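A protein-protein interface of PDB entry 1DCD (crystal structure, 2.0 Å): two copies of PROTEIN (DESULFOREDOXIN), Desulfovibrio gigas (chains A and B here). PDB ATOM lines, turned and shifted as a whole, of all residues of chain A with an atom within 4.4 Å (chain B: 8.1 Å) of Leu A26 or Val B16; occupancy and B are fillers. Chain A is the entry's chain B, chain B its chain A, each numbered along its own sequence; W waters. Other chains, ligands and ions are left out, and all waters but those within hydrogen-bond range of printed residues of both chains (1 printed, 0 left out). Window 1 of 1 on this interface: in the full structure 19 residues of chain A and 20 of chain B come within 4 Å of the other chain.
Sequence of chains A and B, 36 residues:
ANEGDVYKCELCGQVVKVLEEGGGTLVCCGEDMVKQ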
ATOM      1  N   ALA A   1      -9.520  11.616 -32.038  1.00  0.00           N
ATOM      2  CA  ALA A   1     -10.202  10.612 -32.859  1.00  0.00           C
ATOM      3  C   ALA A   1     -11.220  11.304 -33.753  1.00  0.00           C
ATOM      4  O   ALA A   1     -11.352  12.525 -33.659  1.00  0.00           O
ATOM      5  CB  ALA A   1     -10.841   9.561 -31.971  1.00  0.00           C
ATOM      6  N   TYR A   7     -13.896   2.641 -31.616  1.00  0.00           N
ATOM      7  CA  TYR A   7     -12.759   2.307 -30.781  1.00  0.00           C
ATOM      8  C   TYR A   7     -13.062   1.147 -29.833  1.00  0.00           C
ATOM      9  O   TYR A   7     -14.190   0.984 -29.366  1.00  0.00           O
ATOM     10  CB  TYR A   7     -12.349   3.529 -29.955  1.00  0.00           C
ATOM     11  CG  TYR A   7     -11.445   4.493 -30.684  1.00  0.00           C
ATOM     12  CD1 TYR A   7     -11.933   5.393 -31.627  1.00  0.00           C
ATOM     13  CD2 TYR A   7     -10.084   4.505 -30.411  1.00  0.00           C
ATOM     14  CE1 TYR A   7     -11.067   6.267 -32.267  1.00  0.00           C
ATOM     15  CE2 TYR A   7      -9.214   5.368 -31.050  1.00  0.00           C
ATOM     16  CZ  TYR A   7      -9.724   6.251 -31.979  1.00  0.00           C
ATOM     17  OH  TYR A   7      -8.862   7.116 -32.617  1.00  0.00           O
ATOM     18  N   VAL A  16     -16.731   1.646 -28.504  1.00  0.00           N
ATOM     19  CA  VAL A  16     -17.503   2.879 -28.622  1.00  0.00           C
ATOM     20  C   VAL A  16     -17.430   3.482 -30.021  1.00  0.00           C
ATOM     21  O   VAL A  16     -16.438   3.329 -30.736  1.00  0.00           O
ATOM     22  CB  VAL A  16     -17.063   3.968 -27.623  1.00  0.00           C
ATOM     23  CG1 VAL A  16     -17.208   3.486 -26.189  1.00  0.00           C
ATOM     24  CG2 VAL A  16     -15.636   4.412 -27.899  1.00  0.00           C
ATOM     25  N   LYS A  17     -18.474   4.213 -30.381  1.00  0.00           N
ATOM     26  CA  LYS A  17     -18.485   4.988 -31.614  1.00  0.00           C
ATOM     27  C   LYS A  17     -18.331   6.481 -31.320  1.00  0.00           C
ATOM     28  O   LYS A  17     -19.016   7.051 -30.474  1.00  0.00           O
ATOM     29  CB  LYS A  17     -19.780   4.785 -32.413  1.00  0.00           C
ATOM     30  CG  LYS A  17     -19.590   5.172 -33.885  1.00  0.00           C
ATOM     31  CD  LYS A  17     -20.901   5.694 -34.450  1.00  0.00           C
ATOM     32  CE  LYS A  17     -20.691   6.379 -35.799  1.00  0.00           C
ATOM     33  NZ  LYS A  17     -21.435   5.641 -36.862  1.00  0.00           N
ATOM     34  N   VAL A  18     -17.433   7.158 -32.039  1.00  0.00           N
ATOM     35  CA  VAL A  18     -17.288   8.597 -31.803  1.00  0.00           C
ATOM     36  C   VAL A  18     -18.454   9.362 -32.411  1.00  0.00           C
ATOM     37  O   VAL A  18     -18.682   9.327 -33.618  1.00  0.00           O
ATOM     38  CB  VAL A  18     -15.929   9.083 -32.328  1.00  0.00           C
ATOM     39  CG1 VAL A  18     -15.812  10.595 -32.353  1.00  0.00           C
ATOM     40  CG2 VAL A  18     -14.846   8.481 -31.432  1.00  0.00           C
ATOM     41  N   LEU A  19     -19.194  10.038 -31.543  1.00  0.00           N
ATOM     42  CA  LEU A  19     -20.368  10.815 -31.923  1.00  0.00           C
ATOM     43  C   LEU A  19     -19.961  12.264 -32.185  1.00  0.00           C
ATOM     44  O   LEU A  19     -20.405  12.878 -33.152  1.00  0.00           O
ATOM     45  CB  LEU A  19     -21.413  10.775 -30.808  1.00  0.00           C
ATOM     46  CG  LEU A  19     -22.142   9.441 -30.624  1.00  0.00           C
ATOM     47  CD1 LEU A  19     -23.340   9.598 -29.707  1.00  0.00           C
ATOM     48  CD2 LEU A  19     -22.558   8.882 -31.972  1.00  0.00           C
ATOM     49  N   GLY A  24      -8.878  14.808 -27.636  1.00  0.00           N
ATOM     50  CA  GLY A  24      -8.366  13.912 -26.608  1.00  0.00           C
ATOM     51  C   GLY A  24      -8.207  12.487 -27.100  1.00  0.00           C
ATOM     52  O   GLY A  24      -8.882  12.054 -28.033  1.00  0.00           O
ATOM     53  N   THR A  25      -7.332  11.741 -26.453  1.00  0.00           N
ATOM     54  CA  THR A  25      -7.075  10.341 -26.756  1.00  0.00           C
ATOM     55  C   THR A  25      -7.985   9.459 -25.909  1.00  0.00           C
ATOM     56  O   THR A  25      -8.000   9.637 -24.685  1.00  0.00           O
ATOM     57  CB  THR A  25      -5.617  10.007 -26.368  1.00  0.00           C
ATOM     58  OG1 THR A  25      -4.754  10.842 -27.141  1.00  0.00           O
ATOM     59  CG2 THR A  25      -5.286   8.563 -26.716  1.00  0.00           C
ATOM     60  N   LEU A  26      -8.756   8.584 -26.549  1.00  0.00           N
ATOM     61  CA  LEU A  26      -9.727   7.806 -25.786  1.00  0.00           C
ATOM     62  C   LEU A  26      -9.019   6.712 -25.006  1.00  0.00           C
ATOM     63  O   LEU A  26      -8.123   6.044 -25.529  1.00  0.00           O
ATOM     64  CB  LEU A  26     -10.795   7.259 -26.737  1.00  0.00           C
ATOM     65  CG  LEU A  26     -11.791   8.319 -27.218  1.00  0.00           C
ATOM     66  CD1 LEU A  26     -12.434   7.911 -28.531  1.00  0.00           C
ATOM     67  CD2 LEU A  26     -12.843   8.588 -26.145  1.00  0.00           C
ATOM     68  N   VAL A  27      -9.352   6.599 -23.719  1.00  0.00           N
ATOM     69  CA  VAL A  27      -8.648   5.633 -22.870  1.00  0.00           C
ATOM     70  C   VAL A  27      -9.642   4.772 -22.103  1.00  0.00           C
ATOM     71  O   VAL A  27     -10.724   5.176 -21.687  1.00  0.00           O
ATOM     72  CB  VAL A  27      -7.662   6.341 -21.919  1.00  0.00           C
ATOM     73  CG1 VAL A  27      -7.071   5.363 -20.904  1.00  0.00           C
ATOM     74  CG2 VAL A  27      -6.552   7.041 -22.682  1.00  0.00           C
ATOM     75  N   ASP A  32      -4.562   2.919 -24.138  1.00  0.00           N
ATOM     76  CA  ASP A  32      -5.142   3.550 -25.312  1.00  0.00           C
ATOM     77  C   ASP A  32      -6.135   2.629 -26.004  1.00  0.00           C
ATOM     78  O   ASP A  32      -5.796   1.488 -26.322  1.00  0.00           O
ATOM     79  CB  ASP A  32      -4.015   3.908 -26.286  1.00  0.00           C
ATOM     80  CG  ASP A  32      -3.291   5.183 -25.927  1.00  0.00           C
ATOM     81  OD1 ASP A  32      -3.528   5.735 -24.836  1.00  0.00           O
ATOM     82  OD2 ASP A  32      -2.450   5.637 -26.737  1.00  0.00           O
ATOM     83  N   MET A  33      -7.346   3.122 -26.245  1.00  0.00           N
ATOM     84  CA  MET A  33      -8.315   2.341 -27.006  1.00  0.00           C
ATOM     85  C   MET A  33      -7.815   2.233 -28.442  1.00  0.00           C
ATOM     86  O   MET A  33      -7.033   3.077 -28.889  1.00  0.00           O
ATOM     87  CB  MET A  33      -9.696   3.005 -26.971  1.00  0.00           C
ATOM     88  CG  MET A  33     -10.261   3.048 -25.568  1.00  0.00           C
ATOM     89  SD  MET A  33     -11.968   3.543 -25.434  1.00  0.00           S
ATOM     90  CE  MET A  33     -12.835   2.068 -25.948  1.00  0.00           C
ATOM     91  N   GLY B   4     -25.533   1.721 -25.420  1.00  0.00           N
ATOM     92  CA  GLY B   4     -26.445   2.813 -25.725  1.00  0.00           C
ATOM     93  C   GLY B   4     -26.176   4.003 -24.823  1.00  0.00           C
ATOM     94  O   GLY B   4     -26.816   5.045 -24.940  1.00  0.00           O
ATOM     95  N   ASP B   5     -25.228   3.815 -23.902  1.00  0.00           N
ATOM     96  CA  ASP B   5     -24.854   4.924 -23.022  1.00  0.00           C
ATOM     97  C   ASP B   5     -23.996   5.928 -23.794  1.00  0.00           C
ATOM     98  O   ASP B   5     -23.215   5.537 -24.662  1.00  0.00           O
ATOM     99  CB  ASP B   5     -24.121   4.415 -21.789  1.00  0.00           C
ATOM    100  CG  ASP B   5     -25.014   4.053 -20.625  1.00  0.00           C
ATOM    101  OD1 ASP B   5     -26.252   3.980 -20.779  1.00  0.00           O
ATOM    102  OD2 ASP B   5     -24.471   3.820 -19.523  1.00  0.00           O
ATOM    103  N   VAL B   6     -24.143   7.209 -23.478  1.00  0.00           N
ATOM    104  CA  VAL B   6     -23.380   8.282 -24.112  1.00  0.00           C
ATOM    105  C   VAL B   6     -22.482   8.968 -23.087  1.00  0.00           C
ATOM    106  O   VAL B   6     -22.937   9.335 -22.003  1.00  0.00           O
ATOM    107  CB  VAL B   6     -24.332   9.323 -24.739  1.00  0.00           C
ATOM    108  CG1 VAL B   6     -23.562  10.497 -25.315  1.00  0.00           C
ATOM    109  CG2 VAL B   6     -25.205   8.671 -25.803  1.00  0.00           C
ATOM    110  N   TYR B   7     -21.211   9.133 -23.440  1.00  0.00           N
ATOM    111  CA  TYR B   7     -20.212   9.744 -22.575  1.00  0.00           C
ATOM    112  C   TYR B   7     -19.521  10.938 -23.248  1.00  0.00           C
ATOM    113  O   TYR B   7     -19.192  10.897 -24.429  1.00  0.00           O
ATOM    114  CB  TYR B   7     -19.138   8.746 -22.127  1.00  0.00           C
ATOM    115  CG  TYR B   7     -19.626   7.803 -21.043  1.00  0.00           C
ATOM    116  CD1 TYR B   7     -20.425   6.714 -21.373  1.00  0.00           C
ATOM    117  CD2 TYR B   7     -19.292   7.997 -19.713  1.00  0.00           C
ATOM    118  CE1 TYR B   7     -20.889   5.858 -20.393  1.00  0.00           C
ATOM    119  CE2 TYR B   7     -19.741   7.130 -18.729  1.00  0.00           C
ATOM    120  CZ  TYR B   7     -20.547   6.067 -19.074  1.00  0.00           C
ATOM    121  OH  TYR B   7     -21.003   5.196 -18.111  1.00  0.00           O
ATOM    122  N   LYS B   8     -19.298  11.971 -22.444  1.00  0.00           N
ATOM    123  CA  LYS B   8     -18.673  13.204 -22.883  1.00  0.00           C
ATOM    124  C   LYS B   8     -17.511  13.624 -21.992  1.00  0.00           C
ATOM    125  O   LYS B   8     -17.528  13.487 -20.773  1.00  0.00           O
ATOM    126  CB  LYS B   8     -19.707  14.328 -22.956  1.00  0.00           C
ATOM    127  CG  LYS B   8     -19.171  15.709 -23.296  1.00  0.00           C
ATOM    128  CD  LYS B   8     -20.279  16.606 -23.826  1.00  0.00           C
ATOM    129  CE  LYS B   8     -19.793  18.012 -24.103  1.00  0.00           C
ATOM    130  NZ  LYS B   8     -20.815  19.039 -23.762  1.00  0.00           N
ATOM    131  N   CYS B   9     -16.505  14.182 -22.644  1.00  0.00           N
ATOM    132  CA  CYS B   9     -15.352  14.813 -22.025  1.00  0.00           C
ATOM    133  C   CYS B   9     -15.613  16.303 -21.815  1.00  0.00           C
ATOM    134  O   CYS B   9     -15.987  17.056 -22.725  1.00  0.00           O
ATOM    135  CB  CYS B   9     -14.118  14.582 -22.907  1.00  0.00           C
ATOM    136  SG  CYS B   9     -12.637  15.393 -22.251  1.00  0.00           S
ATOM    137  N   CYS B  12     -12.567  18.551 -23.742  1.00  0.00           N
ATOM    138  CA  CYS B  12     -12.454  18.728 -25.184  1.00  0.00           C
ATOM    139  C   CYS B  12     -13.773  18.561 -25.925  1.00  0.00           C
ATOM    140  O   CYS B  12     -13.800  18.775 -27.141  1.00  0.00           O
ATOM    141  CB  CYS B  12     -11.391  17.801 -25.776  1.00  0.00           C
ATOM    142  SG  CYS B  12     -11.922  16.123 -26.187  1.00  0.00           S
ATOM    143  N   GLY B  13     -14.840  18.176 -25.230  1.00  0.00           N
ATOM    144  CA  GLY B  13     -16.150  18.042 -25.841  1.00  0.00           C
ATOM    145  C   GLY B  13     -16.374  16.776 -26.632  1.00  0.00           C
ATOM    146  O   GLY B  13     -17.420  16.633 -27.268  1.00  0.00           O
ATOM    147  N   GLN B  14     -15.422  15.850 -26.614  1.00  0.00           N
ATOM    148  CA  GLN B  14     -15.540  14.583 -27.321  1.00  0.00           C
ATOM    149  C   GLN B  14     -16.699  13.781 -26.736  1.00  0.00           C
ATOM    150  O   GLN B  14     -16.853  13.739 -25.516  1.00  0.00           O
ATOM    151  CB  GLN B  14     -14.241  13.785 -27.243  1.00  0.00           C
ATOM    152  CG  GLN B  14     -14.224  12.527 -28.101  1.00  0.00           C
ATOM    153  CD  GLN B  14     -12.897  12.299 -28.795  1.00  0.00           C
ATOM    154  OE1 GLN B  14     -12.807  12.243 -30.021  1.00  0.00           O
ATOM    155  NE2 GLN B  14     -11.837  12.128 -28.016  1.00  0.00           N
ATOM    156  N   VAL B  15     -17.525  13.258 -27.629  1.00  0.00           N
ATOM    157  CA  VAL B  15     -18.733  12.539 -27.261  1.00  0.00           C
ATOM    158  C   VAL B  15     -18.722  11.158 -27.910  1.00  0.00           C
ATOM    159  O   VAL B  15     -18.521  11.045 -29.118  1.00  0.00           O
ATOM    160  CB  VAL B  15     -20.008  13.280 -27.703  1.00  0.00           C
ATOM    161  CG1 VAL B  15     -21.246  12.532 -27.234  1.00  0.00           C
ATOM    162  CG2 VAL B  15     -20.037  14.712 -27.183  1.00  0.00           C
ATOM    163  N   VAL B  16     -18.920  10.128 -27.094  1.00  0.00           N
ATOM    164  CA  VAL B  16     -18.943   8.760 -27.598  1.00  0.00           C
ATOM    165  C   VAL B  16     -20.205   8.023 -27.156  1.00  0.00           C
ATOM    166  O   VAL B  16     -20.810   8.341 -26.133  1.00  0.00           O
ATOM    167  CB  VAL B  16     -17.723   7.943 -27.144  1.00  0.00           C
ATOM    168  CG1 VAL B  16     -16.421   8.590 -27.577  1.00  0.00           C
ATOM    169  CG2 VAL B  16     -17.728   7.713 -25.640  1.00  0.00           C
ATOM    170  N   LYS B  17     -20.562   6.994 -27.918  1.00  0.00           N
ATOM    171  CA  LYS B  17     -21.661   6.111 -27.529  1.00  0.00           C
ATOM    172  C   LYS B  17     -21.144   4.690 -27.337  1.00  0.00           C
ATOM    173  O   LYS B  17     -20.340   4.196 -28.133  1.00  0.00           O
ATOM    174  CB  LYS B  17     -22.755   6.133 -28.592  1.00  0.00           C
ATOM    175  CG  LYS B  17     -24.155   5.831 -28.092  1.00  0.00           C
ATOM    176  CD  LYS B  17     -24.947   5.030 -29.111  1.00  0.00           C
ATOM    177  CE  LYS B  17     -26.274   5.707 -29.431  1.00  0.00           C
ATOM    178  NZ  LYS B  17     -26.658   5.481 -30.849  1.00  0.00           N
ATOM    179  N   VAL B  18     -21.568   4.013 -26.271  1.00  0.00           N
ATOM    180  CA  VAL B  18     -21.056   2.661 -26.052  1.00  0.00           C
ATOM    181  C   VAL B  18     -21.759   1.664 -26.966  1.00  0.00           C
ATOM    182  O   VAL B  18     -22.973   1.477 -26.880  1.00  0.00           O
ATOM    183  CB  VAL B  18     -21.203   2.219 -24.585  1.00  0.00           C
ATOM    184  CG1 VAL B  18     -20.505   0.884 -24.360  1.00  0.00           C
ATOM    185  CG2 VAL B  18     -20.652   3.274 -23.636  1.00  0.00           C
ATOM    186  N   LEU B  19     -20.998   1.027 -27.857  1.00  0.00           N
ATOM    187  CA  LEU B  19     -21.578   0.015 -28.736  1.00  0.00           C
ATOM    188  C   LEU B  19     -21.591  -1.358 -28.071  1.00  0.00           C
ATOM    189  O   LEU B  19     -22.570  -2.093 -28.158  1.00  0.00           O
ATOM    190  CB  LEU B  19     -20.817  -0.062 -30.058  1.00  0.00           C
ATOM    191  CG  LEU B  19     -20.953   1.141 -30.996  1.00  0.00           C
ATOM    192  CD1 LEU B  19     -20.735   0.720 -32.442  1.00  0.00           C
ATOM    193  CD2 LEU B  19     -22.318   1.790 -30.828  1.00  0.00           C
ATOM    194  N   THR B  25     -13.483   1.927 -17.193  1.00  0.00           N
ATOM    195  CA  THR B  25     -13.981   3.301 -17.111  1.00  0.00           C
ATOM    196  C   THR B  25     -13.456   4.096 -18.296  1.00  0.00           C
ATOM    197  O   THR B  25     -12.248   4.122 -18.506  1.00  0.00           O
ATOM    198  CB  THR B  25     -13.461   3.921 -15.798  1.00  0.00           C
ATOM    199  OG1 THR B  25     -14.128   3.240 -14.726  1.00  0.00           O
ATOM    200  CG2 THR B  25     -13.809   5.391 -15.694  1.00  0.00           C
ATOM    201  N   LEU B  26     -14.342   4.724 -19.049  1.00  0.00           N
ATOM    202  CA  LEU B  26     -13.884   5.496 -20.200  1.00  0.00           C
ATOM    203  C   LEU B  26     -13.186   6.777 -19.763  1.00  0.00           C
ATOM    204  O   LEU B  26     -13.670   7.506 -18.903  1.00  0.00           O
ATOM    205  CB  LEU B  26     -15.057   5.790 -21.140  1.00  0.00           C
ATOM    206  CG  LEU B  26     -15.659   4.552 -21.814  1.00  0.00           C
ATOM    207  CD1 LEU B  26     -17.029   4.869 -22.384  1.00  0.00           C
ATOM    208  CD2 LEU B  26     -14.725   4.012 -22.883  1.00  0.00           C
ATOM    209  N   VAL B  27     -12.027   7.030 -20.355  1.00  0.00           N
ATOM    210  CA  VAL B  27     -11.215   8.201 -20.035  1.00  0.00           C
ATOM    211  C   VAL B  27     -10.886   8.982 -21.301  1.00  0.00           C
ATOM    212  O   VAL B  27     -10.706   8.395 -22.371  1.00  0.00           O
ATOM    213  CB  VAL B  27      -9.951   7.759 -19.281  1.00  0.00           C
ATOM    214  CG1 VAL B  27      -8.864   8.813 -19.212  1.00  0.00           C
ATOM    215  CG2 VAL B  27     -10.345   7.310 -17.872  1.00  0.00           C
ATOM    216  N   CYS B  28     -10.849  10.304 -21.193  1.00  0.00           N
ATOM    217  CA  CYS B  28     -10.461  11.182 -22.295  1.00  0.00           C
ATOM    218  C   CYS B  28      -9.769  12.416 -21.723  1.00  0.00           C
ATOM    219  O   CYS B  28     -10.143  12.907 -20.657  1.00  0.00           O
ATOM    220  CB  CYS B  28     -11.668  11.569 -23.147  1.00  0.00           C
ATOM    221  SG  CYS B  28     -11.273  12.358 -24.729  1.00  0.00           S
ATOM    222  N   CYS B  29      -8.704  12.889 -22.356  1.00  0.00           N
ATOM    223  CA  CYS B  29      -7.869  13.939 -21.800  1.00  0.00           C
ATOM    224  C   CYS B  29      -7.428  13.562 -20.381  1.00  0.00           C
ATOM    225  O   CYS B  29      -7.276  14.455 -19.553  1.00  0.00           O
ATOM    226  CB  CYS B  29      -8.562  15.302 -21.777  1.00  0.00           C
ATOM    227  SG  CYS B  29      -8.945  15.967 -23.416  1.00  0.00           S
ATOM    228  N   GLY B  30      -7.225  12.274 -20.147  1.00  0.00           N
ATOM    229  CA  GLY B  30      -6.799  11.703 -18.884  1.00  0.00           C
ATOM    230  C   GLY B  30      -7.783  11.886 -17.749  1.00  0.00           C
ATOM    231  O   GLY B  30      -7.445  11.670 -16.584  1.00  0.00           O
ATOM    232  N   MET B  33     -14.679  10.167 -18.394  1.00  0.00           N
ATOM    233  CA  MET B  33     -15.764  10.800 -19.152  1.00  0.00           C
ATOM    234  C   MET B  33     -17.018  10.837 -18.288  1.00  0.00           C
ATOM    235  O   MET B  33     -17.168  10.051 -17.358  1.00  0.00           O
ATOM    236  CB  MET B  33     -16.016  10.105 -20.491  1.00  0.00           C
ATOM    237  CG  MET B  33     -14.744  10.008 -21.324  1.00  0.00           C
ATOM    238  SD  MET B  33     -14.991   9.376 -22.981  1.00  0.00           S
ATOM    239  CE  MET B  33     -15.613  10.823 -23.847  1.00  0.00           C
ATOM    240  N   VAL B  34     -17.897  11.780 -18.576  1.00  0.00           N
ATOM    241  CA  VAL B  34     -19.126  11.964 -17.814  1.00  0.00           C
ATOM    242  C   VAL B  34     -20.308  11.291 -18.493  1.00  0.00           C
ATOM    243  O   VAL B  34     -20.579  11.553 -19.667  1.00  0.00           O
ATOM    244  CB  VAL B  34     -19.376  13.479 -17.666  1.00  0.00           C
ATOM    245  CG1 VAL B  34     -20.656  13.792 -16.911  1.00  0.00           C
ATOM    246  CG2 VAL B  34     -18.180  14.098 -16.949  1.00  0.00           C
ATOM    247  N   GLN B  36     -23.708  10.957 -19.797  1.00  0.00           N
ATOM    248  CA  GLN B  36     -24.748  11.904 -20.179  1.00  0.00           C
ATOM    249  C   GLN B  36     -26.130  11.385 -19.810  1.00  0.00           C
ATOM    250  O   GLN B  36     -26.992  12.214 -19.455  1.00  0.00           O
ATOM    251  CB  GLN B  36     -24.632  12.209 -21.670  1.00  0.00           C
ATOM    252  CG  GLN B  36     -23.504  13.167 -22.015  1.00  0.00           C
ATOM    253  CD  GLN B  36     -23.216  14.155 -20.904  1.00  0.00           C
ATOM    254  OE1 GLN B  36     -22.243  14.009 -20.163  1.00  0.00           O
ATOM    255  NE2 GLN B  36     -24.064  15.169 -20.765  1.00  0.00           N
ATOM    256  OXT GLN B  36     -26.350  10.158 -19.835  1.00  0.00           O
HETATM  257  O   HOH W   1      -6.730  10.235 -22.285  1.00  0.00           O
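The side-chain sulfur of Cys B12 lies close to the backbone NH of Gly A24, 3.6 Å away.
O of Gly A24 sits at hydrogen-bond distance from NE2 of Gln B14, at 3.0 Å.
O of Val B15 sits at hydrogen-bond distance from N of Leu A19, at 2.7 Å.
The backbone carbonyl oxygen (O) of Lys B17 lies within hydrogen-bond range of the backbone NH (N) of Lys A17 (2.9 Å).
O of Val B27 sits at hydrogen-bond distance from N of Val A27, 2.6 Å away.
The backbone carbonyl oxygen of Asp B5 lies within hydrogen-bond range of the backbone NH of Val B18, at 2.8 Å.
N of Val B16 lies within hydrogen-bond range of O of Tyr B7.
The backbone NH (N) of Gln B14 sits close to the side-chain sulfur (SG) of Cys B12.
The backbone carbonyl oxygen of Leu B26 sits at hydrogen-bond distance from the backbone NH of Met B33 (2.9 Å).
N of Val A16 is in hydrogen-bond range of O of Tyr A7.
The backbone carbonyl oxygen (O) of Leu A26 is in hydrogen-bond range of the backbone NH (N) of Met A33 (3.1 Å).
Val A16 touches Lys B17 (CA to O, 3.2 Å).
Leu B19 touches Lys A17.
Leu A19 touches Lys B17.
Gly A24 touches Cys B28.
Cys B29 touches Gly A24 (SG to CA, 3.8 Å).
Leu A26 touches Val B16.
Val B27 touches Leu A26 (O to C, 3.6 Å).
Leu A26 touches Met B33.
Thr B25 touches Val A27.
O of Val A27 touches CA of Leu B26 (3.5 Å).
Leu A26 touches four residues of chain B.
Of the printed residues of chain A, Cys B28 touches Gly A24 and Thr A25.
Of the printed residues of chain B, Gly A24 touches Cys B12, Gln B14, Cys B28 and Cys B29.
Val B6 touches none of the printed residues of chain A.
The nearest residue of chain B that does not touch Leu A26 is Cys B28 (4.3 Å).
Of the 12 printed residues of chain A, 10 touch a printed residue of chain B.
Hydrophobic or aromatic side chains of chain A within 4 Å of the printed part of chain B: Ala A1, Val A16, Leu A19, Leu A26, Val A27 and Met A33.
Hydrophobic or aromatic side chains of chain B within 4 Å of the printed part of chain A: Val B15, Val B16, Leu B19, Leu B26, Val B27 and Met B33.
Along chain B the printed residues that touch a printed residue of chain A span positions 12 to 33.
Among the printed residues, 23 pairs touch across the chains.
Among the printed residues, no Asp or Glu carboxylate lies within 4 Å of a Lys or Arg side-chain nitrogen of the other chain.
Lys A17 touches its own counterpart, Lys B17.
Thr A25 touches Val B27, and with the chains exchanged Val A27 touches Thr B25.
Leu A26 touches Val B27, and with the chains exchanged Val A27 touches Leu B26.
Leu A26 touches Met B33, and with the chains exchanged Met A33 touches Leu B26.
9 positions are printed for both chains.
Water W1 lies within hydrogen-bond range of the backbone carbonyl oxygen (O) of Thr A25 (2.8 Å), the backbone NH (N) of Gly B30 (3.0 Å) and the backbone NH (N) of Cys B29 (3.3 Å).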
